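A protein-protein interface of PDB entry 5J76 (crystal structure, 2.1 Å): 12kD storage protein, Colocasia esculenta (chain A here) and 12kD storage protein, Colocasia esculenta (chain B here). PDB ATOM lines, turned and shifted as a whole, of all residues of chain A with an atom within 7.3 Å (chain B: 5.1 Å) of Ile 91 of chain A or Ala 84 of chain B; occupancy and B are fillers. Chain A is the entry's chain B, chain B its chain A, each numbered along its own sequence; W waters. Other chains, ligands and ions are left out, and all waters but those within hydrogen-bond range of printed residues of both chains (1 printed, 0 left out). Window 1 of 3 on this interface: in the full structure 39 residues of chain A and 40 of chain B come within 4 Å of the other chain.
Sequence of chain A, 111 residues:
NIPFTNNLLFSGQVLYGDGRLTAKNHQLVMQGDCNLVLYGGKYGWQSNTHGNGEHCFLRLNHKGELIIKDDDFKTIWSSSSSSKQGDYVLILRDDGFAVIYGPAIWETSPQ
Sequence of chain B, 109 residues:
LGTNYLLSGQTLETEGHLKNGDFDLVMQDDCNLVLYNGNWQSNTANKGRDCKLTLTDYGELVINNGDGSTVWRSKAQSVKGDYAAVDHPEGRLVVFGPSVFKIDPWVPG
Water W1 bridges O of Tyr 83 of chain B and OH of Tyr 101 of chain A.
O of Ala 84 of chain B sits at hydrogen-bond distance from N of Phe 96 of chain B. The backbone carbonyl oxygen (O) of Val 94 of chain B sits at hydrogen-bond distance from the backbone NH (N) of Val 86 of chain B (2.9 Å). The backbone carbonyl oxygen (O) of Asn 7 of chain A is in hydrogen-bond range of the backbone NH (N) of Leu 92 of chain A, 3.0 Å away. The backbone carbonyl oxygen (O) of Val 89 of chain A is in hydrogen-bond range of the backbone NH (N) of Tyr 101 of chain A, at 2.9 Å. N of Ile 91 of chain A is in hydrogen-bond range of O of Val 99 of chain A (2.8 Å). The guanidinium group of Arg 93 of chain A is in salt-bridge range of the side-chain carboxylate of Asp 95 of chain A, at 2.6 Å.
ND2 of Asn 7 of chain A touches CE2 of Tyr 5 of chain B (3.6 Å). CD1 of Leu 8 of chain A touches CG1 of Val 86 of chain B, 3.6 Å away. CE1 of Phe 10 of chain A touches CZ of Phe 96 of chain B (3.7 Å). CG1 of Val 89 of chain A touches CD1 of Phe 96 of chain B, 3.7 Å away. Ile 91 of chain A touches Ala 84 of chain B. Leu 7 of chain B touches Arg 93 of chain A (CD1 to NE, 3.9 Å). Leu 7 of chain B touches Tyr 101 of chain A (CD2 to OH, 3.6 Å). Asp 82 of chain B touches Tyr 101 of chain A. Tyr 83 of chain B touches Tyr 101 of chain A (C to CE2, 3.7 Å). Ala 84 of chain B touches Tyr 101 of chain A.
Of the 22 printed residues of chain A, 8 touch a printed residue of chain B. Along chain A the printed residues that touch a printed residue of chain B span positions 7 to 101. Among the printed residues, 15 pairs touch across the chains. Among the printed residues, no Asp or Glu carboxylate lies within 4 Å of a Lys or Arg side-chain nitrogen of the other chain.
Of the printed residues of chain B, Asn 7 of chain A touches Tyr 5 (3.6 Å). Leu 28 of chain A touches none of the printed residues of chain B. Ile 91 of chain A touches two residues of chain B. Gly 102 of chain A touches none of the printed residues of chain B. Of the printed residues of chain A, Tyr 5 of chain B touches Asn 7, Arg 93 and Asp 94. Of the printed residues of chain A, Tyr 83 of chain B touches Tyr 101 (3.7 Å). Of the printed residues of chain A, Val 86 of chain B touches Leu 8, Phe 10 and Ile 91. Of the printed residues of chain A, Phe 96 of chain B touches Phe 10 (3.7 Å), Val 89 (3.7 Å) and Tyr 101 (3.7 Å). The nearest residue of chain A that does not touch Ala 84 of chain B is Val 89 of chain A (5.6 Å).
The backbone NH (N) of Asp 94 of chain A is in hydrogen-bond range of the side-chain hydroxyl (OH) of Tyr 5 of chain B (3.1 Å).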
ATOM      1  N   ASN A   7     -11.063  13.297   8.844  1.00  0.00           N
ATOM      2  CA  ASN A   7      -9.767  13.375   9.486  1.00  0.00           C
ATOM      3  C   ASN A   7      -9.730  12.673  10.805  1.00  0.00           C
ATOM      4  O   ASN A   7      -8.746  12.772  11.437  1.00  0.00           O
ATOM      5  CB  ASN A   7      -9.316  14.827   9.627  1.00  0.00           C
ATOM      6  CG  ASN A   7     -10.225  15.650  10.503  1.00  0.00           C
ATOM      7  OD1 ASN A   7     -11.405  15.395  10.603  1.00  0.00           O
ATOM      8  ND2 ASN A   7      -9.681  16.645  11.127  1.00  0.00           N
ATOM      9  N   LEU A   8     -10.811  11.976  11.184  1.00  0.00           N
ATOM     10  CA  LEU A   8     -10.942  11.280  12.452  1.00  0.00           C
ATOM     11  C   LEU A   8     -11.322   9.808  12.344  1.00  0.00           C
ATOM     12  O   LEU A   8     -12.048   9.385  11.460  1.00  0.00           O
ATOM     13  CB  LEU A   8     -12.029  11.895  13.291  1.00  0.00           C
ATOM     14  CG  LEU A   8     -12.028  13.439  13.416  1.00  0.00           C
ATOM     15  CD1 LEU A   8     -13.288  13.953  14.137  1.00  0.00           C
ATOM     16  CD2 LEU A   8     -10.836  13.996  14.146  1.00  0.00           C
ATOM     17  N   LEU A   9     -10.875   9.033  13.322  1.00  0.00           N
ATOM     18  CA  LEU A   9     -11.295   7.686  13.533  1.00  0.00           C
ATOM     19  C   LEU A   9     -11.458   7.461  15.045  1.00  0.00           C
ATOM     20  O   LEU A   9     -10.504   7.460  15.792  1.00  0.00           O
ATOM     21  CB  LEU A   9     -10.300   6.730  12.971  1.00  0.00           C
ATOM     22  CG  LEU A   9     -10.904   5.319  12.819  1.00  0.00           C
ATOM     23  CD1 LEU A   9     -11.813   5.201  11.594  1.00  0.00           C
ATOM     24  CD2 LEU A   9      -9.785   4.277  12.668  1.00  0.00           C
ATOM     25  N   PHE A  10     -12.696   7.347  15.476  1.00  0.00           N
ATOM     26  CA  PHE A  10     -13.044   7.078  16.873  1.00  0.00           C
ATOM     27  C   PHE A  10     -13.025   5.606  17.182  1.00  0.00           C
ATOM     28  O   PHE A  10     -13.101   4.766  16.246  1.00  0.00           O
ATOM     29  CB  PHE A  10     -14.405   7.635  17.242  1.00  0.00           C
ATOM     30  CG  PHE A  10     -14.512   9.147  17.165  1.00  0.00           C
ATOM     31  CD1 PHE A  10     -14.026   9.950  18.181  1.00  0.00           C
ATOM     32  CD2 PHE A  10     -15.055   9.757  16.056  1.00  0.00           C
ATOM     33  CE1 PHE A  10     -14.098  11.330  18.126  1.00  0.00           C
ATOM     34  CE2 PHE A  10     -15.161  11.148  15.999  1.00  0.00           C
ATOM     35  CZ  PHE A  10     -14.683  11.948  17.013  1.00  0.00           C
ATOM     36  N   LEU A  21      -8.336   8.177   6.075  1.00  0.00           N
ATOM     37  CA  LEU A  21      -8.470   9.503   6.611  1.00  0.00           C
ATOM     38  C   LEU A  21      -7.763  10.445   5.646  1.00  0.00           C
ATOM     39  O   LEU A  21      -6.765  10.089   5.016  1.00  0.00           O
ATOM     40  CB  LEU A  21      -7.770   9.611   7.996  1.00  0.00           C
ATOM     41  CG  LEU A  21      -8.264   8.622   9.069  1.00  0.00           C
ATOM     42  CD1 LEU A  21      -7.796   8.997  10.478  1.00  0.00           C
ATOM     43  CD2 LEU A  21      -9.781   8.537   9.013  1.00  0.00           C
ATOM     44  N   ALA A  23      -6.627  14.693   5.261  1.00  0.00           N
ATOM     45  CA  ALA A  23      -6.481  16.040   5.777  1.00  0.00           C
ATOM     46  C   ALA A  23      -5.589  16.817   4.785  1.00  0.00           C
ATOM     47  O   ALA A  23      -5.344  16.389   3.654  1.00  0.00           O
ATOM     48  CB  ALA A  23      -5.854  15.982   7.165  1.00  0.00           C
ATOM     49  N   LEU A  28      -4.207   8.830   5.106  1.00  0.00           N
ATOM     50  CA  LEU A  28      -3.779   7.592   5.859  1.00  0.00           C
ATOM     51  C   LEU A  28      -4.735   6.497   5.340  1.00  0.00           C
ATOM     52  O   LEU A  28      -5.923   6.565   5.670  1.00  0.00           O
ATOM     53  CB  LEU A  28      -3.935   7.807   7.344  1.00  0.00           C
ATOM     54  CG  LEU A  28      -3.595   6.576   8.203  1.00  0.00           C
ATOM     55  CD1 LEU A  28      -2.124   6.138   7.948  1.00  0.00           C
ATOM     56  CD2 LEU A  28      -3.908   6.895   9.671  1.00  0.00           C
ATOM     57  N   LEU A  60      -9.506   1.011  15.815  1.00  0.00           N
ATOM     58  CA  LEU A  60      -9.082   1.579  17.088  1.00  0.00           C
ATOM     59  C   LEU A  60      -9.969   1.077  18.195  1.00  0.00           C
ATOM     60  O   LEU A  60     -11.163   1.156  18.092  1.00  0.00           O
ATOM     61  CB  LEU A  60      -9.150   3.107  17.038  1.00  0.00           C
ATOM     62  CG  LEU A  60      -8.686   3.854  18.272  1.00  0.00           C
ATOM     63  CD1 LEU A  60      -7.232   3.538  18.570  1.00  0.00           C
ATOM     64  CD2 LEU A  60      -8.848   5.364  18.071  1.00  0.00           C
ATOM     65  N   VAL A  89      -9.498   8.634  20.043  1.00  0.00           N
ATOM     66  CA  VAL A  89      -9.602   9.164  18.667  1.00  0.00           C
ATOM     67  C   VAL A  89      -8.271   9.250  18.020  1.00  0.00           C
ATOM     68  O   VAL A  89      -7.299   9.647  18.668  1.00  0.00           O
ATOM     69  CB  VAL A  89     -10.316  10.545  18.638  1.00  0.00           C
ATOM     70  CG1 VAL A  89      -9.541  11.640  19.328  1.00  0.00           C
ATOM     71  CG2 VAL A  89     -10.683  10.929  17.201  1.00  0.00           C
ATOM     72  N   LEU A  90      -8.233   8.814  16.767  1.00  0.00           N
ATOM     73  CA  LEU A  90      -7.069   8.929  15.919  1.00  0.00           C
ATOM     74  C   LEU A  90      -7.346  10.157  15.091  1.00  0.00           C
ATOM     75  O   LEU A  90      -8.399  10.224  14.422  1.00  0.00           O
ATOM     76  CB  LEU A  90      -6.887   7.689  15.020  1.00  0.00           C
ATOM     77  CG  LEU A  90      -5.930   7.807  13.829  1.00  0.00           C
ATOM     78  CD1 LEU A  90      -4.494   8.025  14.365  1.00  0.00           C
ATOM     79  CD2 LEU A  90      -5.957   6.526  12.986  1.00  0.00           C
ATOM     80  N   ILE A  91      -6.451  11.143  15.134  1.00  0.00           N
ATOM     81  CA  ILE A  91      -6.606  12.354  14.319  1.00  0.00           C
ATOM     82  C   ILE A  91      -5.491  12.373  13.291  1.00  0.00           C
ATOM     83  O   ILE A  91      -4.321  12.250  13.642  1.00  0.00           O
ATOM     84  CB  ILE A  91      -6.592  13.607  15.178  1.00  0.00           C
ATOM     85  CG1 ILE A  91      -7.669  13.610  16.279  1.00  0.00           C
ATOM     86  CG2 ILE A  91      -6.805  14.848  14.300  1.00  0.00           C
ATOM     87  CD1 ILE A  91      -7.577  14.802  17.207  1.00  0.00           C
ATOM     88  N   LEU A  92      -5.838  12.500  12.011  1.00  0.00           N
ATOM     89  CA  LEU A  92      -4.863  12.797  10.972  1.00  0.00           C
ATOM     90  C   LEU A  92      -4.885  14.314  10.913  1.00  0.00           C
ATOM     91  O   LEU A  92      -5.807  14.921  10.400  1.00  0.00           O
ATOM     92  CB  LEU A  92      -5.202  12.254   9.609  1.00  0.00           C
ATOM     93  CG  LEU A  92      -4.183  12.554   8.510  1.00  0.00           C
ATOM     94  CD1 LEU A  92      -2.785  12.068   8.859  1.00  0.00           C
ATOM     95  CD2 LEU A  92      -4.582  11.954   7.155  1.00  0.00           C
ATOM     96  N   ARG A  93      -3.881  14.888  11.534  1.00  0.00           N
ATOM     97  CA  ARG A  93      -3.819  16.348  11.775  1.00  0.00           C
ATOM     98  C   ARG A  93      -3.381  17.077  10.531  1.00  0.00           C
ATOM     99  O   ARG A  93      -2.702  16.520   9.674  1.00  0.00           O
ATOM    100  CB  ARG A  93      -2.815  16.642  12.892  1.00  0.00           C
ATOM    101  CG  ARG A  93      -3.327  16.272  14.261  1.00  0.00           C
ATOM    102  CD  ARG A  93      -2.356  16.283  15.431  1.00  0.00           C
ATOM    103  NE  ARG A  93      -1.158  17.032  15.187  1.00  0.00           N
ATOM    104  CZ  ARG A  93      -0.184  17.146  16.087  1.00  0.00           C
ATOM    105  NH1 ARG A  93      -0.319  16.603  17.282  1.00  0.00           N
ATOM    106  NH2 ARG A  93       0.936  17.810  15.802  1.00  0.00           N
ATOM    107  N   ASP A  94      -3.779  18.329  10.451  1.00  0.00           N
ATOM    108  CA  ASP A  94      -3.409  19.224   9.328  1.00  0.00           C
ATOM    109  C   ASP A  94      -1.887  19.383   9.131  1.00  0.00           C
ATOM    110  O   ASP A  94      -1.464  19.649   8.032  1.00  0.00           O
ATOM    111  CB  ASP A  94      -4.064  20.605   9.529  1.00  0.00           C
ATOM    112  CG  ASP A  94      -5.561  20.576   9.313  1.00  0.00           C
ATOM    113  OD1 ASP A  94      -6.040  19.673   8.572  1.00  0.00           O
ATOM    114  OD2 ASP A  94      -6.228  21.474   9.866  1.00  0.00           O
ATOM    115  N   ASP A  95      -1.090  19.191  10.183  1.00  0.00           N
ATOM    116  CA  ASP A  95       0.366  19.117  10.013  1.00  0.00           C
ATOM    117  C   ASP A  95       0.927  17.741   9.601  1.00  0.00           C
ATOM    118  O   ASP A  95       2.110  17.588   9.630  1.00  0.00           O
ATOM    119  CB  ASP A  95       1.056  19.626  11.290  1.00  0.00           C
ATOM    120  CG  ASP A  95       0.815  18.734  12.449  1.00  0.00           C
ATOM    121  OD1 ASP A  95       0.181  17.656  12.337  1.00  0.00           O
ATOM    122  OD2 ASP A  95       1.298  19.078  13.519  1.00  0.00           O
ATOM    123  N   GLY A  96       0.120  16.729   9.240  1.00  0.00           N
ATOM    124  CA  GLY A  96       0.685  15.462   8.739  1.00  0.00           C
ATOM    125  C   GLY A  96       0.878  14.344   9.748  1.00  0.00           C
ATOM    126  O   GLY A  96       0.937  13.145   9.366  1.00  0.00           O
ATOM    127  N   PHE A  97       0.931  14.701  11.031  1.00  0.00           N
ATOM    128  CA  PHE A  97       1.046  13.716  12.110  1.00  0.00           C
ATOM    129  C   PHE A  97      -0.326  13.033  12.306  1.00  0.00           C
ATOM    130  O   PHE A  97      -1.350  13.709  12.184  1.00  0.00           O
ATOM    131  CB  PHE A  97       1.414  14.414  13.415  1.00  0.00           C
ATOM    132  CG  PHE A  97       2.880  14.769  13.539  1.00  0.00           C
ATOM    133  CD1 PHE A  97       3.787  13.874  14.088  1.00  0.00           C
ATOM    134  CD2 PHE A  97       3.354  16.019  13.124  1.00  0.00           C
ATOM    135  CE1 PHE A  97       5.154  14.213  14.216  1.00  0.00           C
ATOM    136  CE2 PHE A  97       4.724  16.375  13.263  1.00  0.00           C
ATOM    137  CZ  PHE A  97       5.624  15.466  13.795  1.00  0.00           C
ATOM    138  N   ALA A  98      -0.332  11.709  12.478  1.00  0.00           N
ATOM    139  CA  ALA A  98      -1.498  10.942  12.888  1.00  0.00           C
ATOM    140  C   ALA A  98      -1.243  10.557  14.333  1.00  0.00           C
ATOM    141  O   ALA A  98      -0.220   9.960  14.649  1.00  0.00           O
ATOM    142  CB  ALA A  98      -1.624   9.701  12.053  1.00  0.00           C
ATOM    143  N   VAL A  99      -2.120  10.983  15.200  1.00  0.00           N
ATOM    144  CA  VAL A  99      -1.968  10.898  16.624  1.00  0.00           C
ATOM    145  C   VAL A  99      -3.216  10.316  17.280  1.00  0.00           C
ATOM    146  O   VAL A  99      -4.344  10.718  16.975  1.00  0.00           O
ATOM    147  CB  VAL A  99      -1.720  12.283  17.228  1.00  0.00           C
ATOM    148  CG1 VAL A  99      -1.416  12.182  18.741  1.00  0.00           C
ATOM    149  CG2 VAL A  99      -0.584  12.982  16.483  1.00  0.00           C
ATOM    150  N   ILE A 100      -3.009   9.367  18.210  1.00  0.00           N
ATOM    151  CA  ILE A 100      -4.065   8.779  18.969  1.00  0.00           C
ATOM    152  C   ILE A 100      -4.114   9.520  20.279  1.00  0.00           C
ATOM    153  O   ILE A 100      -3.091   9.641  20.947  1.00  0.00           O
ATOM    154  CB  ILE A 100      -3.813   7.275  19.224  1.00  0.00           C
ATOM    155  CG1 ILE A 100      -3.743   6.492  17.918  1.00  0.00           C
ATOM    156  CG2 ILE A 100      -4.925   6.739  20.098  1.00  0.00           C
ATOM    157  CD1 ILE A 100      -3.360   5.016  18.094  1.00  0.00           C
ATOM    158  N   TYR A 101      -5.247  10.135  20.592  1.00  0.00           N
ATOM    159  CA  TYR A 101      -5.495  10.779  21.864  1.00  0.00           C
ATOM    160  C   TYR A 101      -6.573  10.062  22.598  1.00  0.00           C
ATOM    161  O   TYR A 101      -7.639   9.698  22.008  1.00  0.00           O
ATOM    162  CB  TYR A 101      -5.999  12.190  21.659  1.00  0.00           C
ATOM    163  CG  TYR A 101      -5.056  13.151  21.005  1.00  0.00           C
ATOM    164  CD1 TYR A 101      -5.039  13.291  19.648  1.00  0.00           C
ATOM    165  CD2 TYR A 101      -4.233  13.964  21.747  1.00  0.00           C
ATOM    166  CE1 TYR A 101      -4.232  14.192  19.037  1.00  0.00           C
ATOM    167  CE2 TYR A 101      -3.431  14.924  21.135  1.00  0.00           C
ATOM    168  CZ  TYR A 101      -3.437  15.033  19.780  1.00  0.00           C
ATOM    169  OH  TYR A 101      -2.614  15.900  19.121  1.00  0.00           O
ATOM    170  N   GLY A 102      -6.364   9.910  23.900  1.00  0.00           N
ATOM    171  CA  GLY A 102      -7.449   9.520  24.789  1.00  0.00           C
ATOM    172  C   GLY A 102      -6.872   9.075  26.131  1.00  0.00           C
ATOM    173  O   GLY A 102      -5.666   9.028  26.264  1.00  0.00           O
ATOM    174  N   TYR B   5     -11.176  20.337  15.370  1.00  0.00           N
ATOM    175  CA  TYR B   5     -10.455  20.055  16.616  1.00  0.00           C
ATOM    176  C   TYR B   5      -9.610  21.229  17.042  1.00  0.00           C
ATOM    177  O   TYR B   5      -9.221  22.052  16.228  1.00  0.00           O
ATOM    178  CB  TYR B   5      -9.548  18.836  16.478  1.00  0.00           C
ATOM    179  CG  TYR B   5      -8.411  18.972  15.480  1.00  0.00           C
ATOM    180  CD1 TYR B   5      -7.199  19.517  15.869  1.00  0.00           C
ATOM    181  CD2 TYR B   5      -8.544  18.529  14.141  1.00  0.00           C
ATOM    182  CE1 TYR B   5      -6.154  19.651  14.974  1.00  0.00           C
ATOM    183  CE2 TYR B   5      -7.527  18.676  13.252  1.00  0.00           C
ATOM    184  CZ  TYR B   5      -6.329  19.235  13.687  1.00  0.00           C
ATOM    185  OH  TYR B   5      -5.312  19.383  12.868  1.00  0.00           O
ATOM    186  N   LEU B   6      -9.376  21.307  18.349  1.00  0.00           N
ATOM    187  CA  LEU B   6      -8.452  22.279  18.925  1.00  0.00           C
ATOM    188  C   LEU B   6      -7.414  21.519  19.771  1.00  0.00           C
ATOM    189  O   LEU B   6      -7.776  20.709  20.635  1.00  0.00           O
ATOM    190  CB  LEU B   6      -9.246  23.277  19.784  1.00  0.00           C
ATOM    191  CG  LEU B   6      -8.458  24.431  20.484  1.00  0.00           C
ATOM    192  CD1 LEU B   6      -8.061  25.504  19.526  1.00  0.00           C
ATOM    193  CD2 LEU B   6      -9.225  25.095  21.608  1.00  0.00           C
ATOM    194  N   LEU B   7      -6.132  21.787  19.536  1.00  0.00           N
ATOM    195  CA  LEU B   7      -5.046  21.121  20.252  1.00  0.00           C
ATOM    196  C   LEU B   7      -4.551  21.966  21.399  1.00  0.00           C
ATOM    197  O   LEU B   7      -4.664  23.160  21.376  1.00  0.00           O
ATOM    198  CB  LEU B   7      -3.868  20.802  19.334  1.00  0.00           C
ATOM    199  CG  LEU B   7      -4.179  19.988  18.086  1.00  0.00           C
ATOM    200  CD1 LEU B   7      -2.897  19.718  17.354  1.00  0.00           C
ATOM    201  CD2 LEU B   7      -4.821  18.656  18.386  1.00  0.00           C
ATOM    202  N   SER B   8      -4.065  21.291  22.411  1.00  0.00           N
ATOM    203  CA  SER B   8      -3.285  21.851  23.522  1.00  0.00           C
ATOM    204  C   SER B   8      -2.336  22.880  23.042  1.00  0.00           C
ATOM    205  O   SER B   8      -1.484  22.527  22.245  1.00  0.00           O
ATOM    206  CB  SER B   8      -2.402  20.699  24.052  1.00  0.00           C
ATOM    207  OG  SER B   8      -3.019  20.211  25.163  1.00  0.00           O
ATOM    208  N   LEU B  55      -6.807  25.320  25.411  1.00  0.00           N
ATOM    209  CA  LEU B  55      -6.849  24.020  26.012  1.00  0.00           C
ATOM    210  C   LEU B  55      -5.496  23.762  26.707  1.00  0.00           C
ATOM    211  O   LEU B  55      -4.493  23.835  26.054  1.00  0.00           O
ATOM    212  CB  LEU B  55      -7.055  23.004  24.855  1.00  0.00           C
ATOM    213  CG  LEU B  55      -6.966  21.525  25.194  1.00  0.00           C
ATOM    214  CD1 LEU B  55      -7.945  21.266  26.288  1.00  0.00           C
ATOM    215  CD2 LEU B  55      -7.278  20.578  23.993  1.00  0.00           C
ATOM    216  N   ASP B  82      -0.180  16.168  25.734  1.00  0.00           N
ATOM    217  CA  ASP B  82      -0.879  16.738  24.582  1.00  0.00           C
ATOM    218  C   ASP B  82      -2.320  16.244  24.545  1.00  0.00           C
ATOM    219  O   ASP B  82      -2.586  15.014  24.629  1.00  0.00           O
ATOM    220  CB  ASP B  82      -0.210  16.290  23.323  1.00  0.00           C
ATOM    221  CG  ASP B  82       1.274  16.654  23.283  1.00  0.00           C
ATOM    222  OD1 ASP B  82       1.625  17.790  23.545  1.00  0.00           O
ATOM    223  OD2 ASP B  82       2.071  15.785  22.919  1.00  0.00           O
ATOM    224  N   TYR B  83      -3.227  17.203  24.437  1.00  0.00           N
ATOM    225  CA  TYR B  83      -4.650  16.944  24.366  1.00  0.00           C
ATOM    226  C   TYR B  83      -5.252  17.476  23.052  1.00  0.00           C
ATOM    227  O   TYR B  83      -4.688  18.324  22.370  1.00  0.00           O
ATOM    228  CB  TYR B  83      -5.339  17.594  25.593  1.00  0.00           C
ATOM    229  CG  TYR B  83      -5.039  16.852  26.859  1.00  0.00           C
ATOM    230  CD1 TYR B  83      -3.822  17.050  27.536  1.00  0.00           C
ATOM    231  CD2 TYR B  83      -5.904  15.904  27.335  1.00  0.00           C
ATOM    232  CE1 TYR B  83      -3.514  16.298  28.677  1.00  0.00           C
ATOM    233  CE2 TYR B  83      -5.635  15.171  28.480  1.00  0.00           C
ATOM    234  CZ  TYR B  83      -4.406  15.368  29.146  1.00  0.00           C
ATOM    235  OH  TYR B  83      -4.135  14.585  30.232  1.00  0.00           O
ATOM    236  N   ALA B  84      -6.472  17.023  22.786  1.00  0.00           N
ATOM    237  CA  ALA B  84      -7.260  17.531  21.652  1.00  0.00           C
ATOM    238  C   ALA B  84      -8.705  17.547  22.064  1.00  0.00           C
ATOM    239  O   ALA B  84      -9.242  16.549  22.608  1.00  0.00           O
ATOM    240  CB  ALA B  84      -7.056  16.575  20.462  1.00  0.00           C
ATOM    241  N   ALA B  85      -9.330  18.684  21.818  1.00  0.00           N
ATOM    242  CA  ALA B  85     -10.759  18.851  21.923  1.00  0.00           C
ATOM    243  C   ALA B  85     -11.306  18.706  20.539  1.00  0.00           C
ATOM    244  O   ALA B  85     -10.989  19.472  19.684  1.00  0.00           O
ATOM    245  CB  ALA B  85     -11.098  20.235  22.481  1.00  0.00           C
ATOM    246  N   VAL B  86     -12.202  17.773  20.365  1.00  0.00           N
ATOM    247  CA  VAL B  86     -12.753  17.396  19.091  1.00  0.00           C
ATOM    248  C   VAL B  86     -14.275  17.506  19.072  1.00  0.00           C
ATOM    249  O   VAL B  86     -14.962  17.174  20.029  1.00  0.00           O
ATOM    250  CB  VAL B  86     -12.394  15.917  18.814  1.00  0.00           C
ATOM    251  CG1 VAL B  86     -12.954  15.463  17.423  1.00  0.00           C
ATOM    252  CG2 VAL B  86     -10.874  15.756  18.941  1.00  0.00           C
ATOM    253  N   VAL B  94     -15.607  16.948  22.919  1.00  0.00           N
ATOM    254  CA  VAL B  94     -15.026  16.013  23.809  1.00  0.00           C
ATOM    255  C   VAL B  94     -13.537  16.321  23.889  1.00  0.00           C
ATOM    256  O   VAL B  94     -12.897  16.538  22.851  1.00  0.00           O
ATOM    257  CB  VAL B  94     -15.208  14.606  23.255  1.00  0.00           C
ATOM    258  CG1 VAL B  94     -14.605  13.586  24.210  1.00  0.00           C
ATOM    259  CG2 VAL B  94     -16.716  14.353  22.964  1.00  0.00           C
ATOM    260  N   VAL B  95     -12.995  16.357  25.106  1.00  0.00           N
ATOM    261  CA  VAL B  95     -11.523  16.507  25.335  1.00  0.00           C
ATOM    262  C   VAL B  95     -10.925  15.116  25.472  1.00  0.00           C
ATOM    263  O   VAL B  95     -11.386  14.342  26.304  1.00  0.00           O
ATOM    264  CB  VAL B  95     -11.156  17.362  26.553  1.00  0.00           C
ATOM    265  CG1 VAL B  95      -9.639  17.513  26.681  1.00  0.00           C
ATOM    266  CG2 VAL B  95     -11.790  18.732  26.421  1.00  0.00           C
ATOM    267  N   PHE B  96      -9.982  14.766  24.573  1.00  0.00           N
ATOM    268  CA  PHE B  96      -9.295  13.493  24.602  1.00  0.00           C
ATOM    269  C   PHE B  96      -7.827  13.739  24.910  1.00  0.00           C
ATOM    270  O   PHE B  96      -7.195  14.661  24.337  1.00  0.00           O
ATOM    271  CB  PHE B  96      -9.326  12.832  23.257  1.00  0.00           C
ATOM    272  CG  PHE B  96     -10.666  12.390  22.808  1.00  0.00           C
ATOM    273  CD1 PHE B  96     -11.465  13.245  22.066  1.00  0.00           C
ATOM    274  CD2 PHE B  96     -11.042  11.068  22.932  1.00  0.00           C
ATOM    275  CE1 PHE B  96     -12.699  12.815  21.558  1.00  0.00           C
ATOM    276  CE2 PHE B  96     -12.283  10.631  22.450  1.00  0.00           C
ATOM    277  CZ  PHE B  96     -13.105  11.526  21.731  1.00  0.00           C
HETATM  278  O   HOH W   1      -2.182  17.912  21.141  1.00  0.00           O
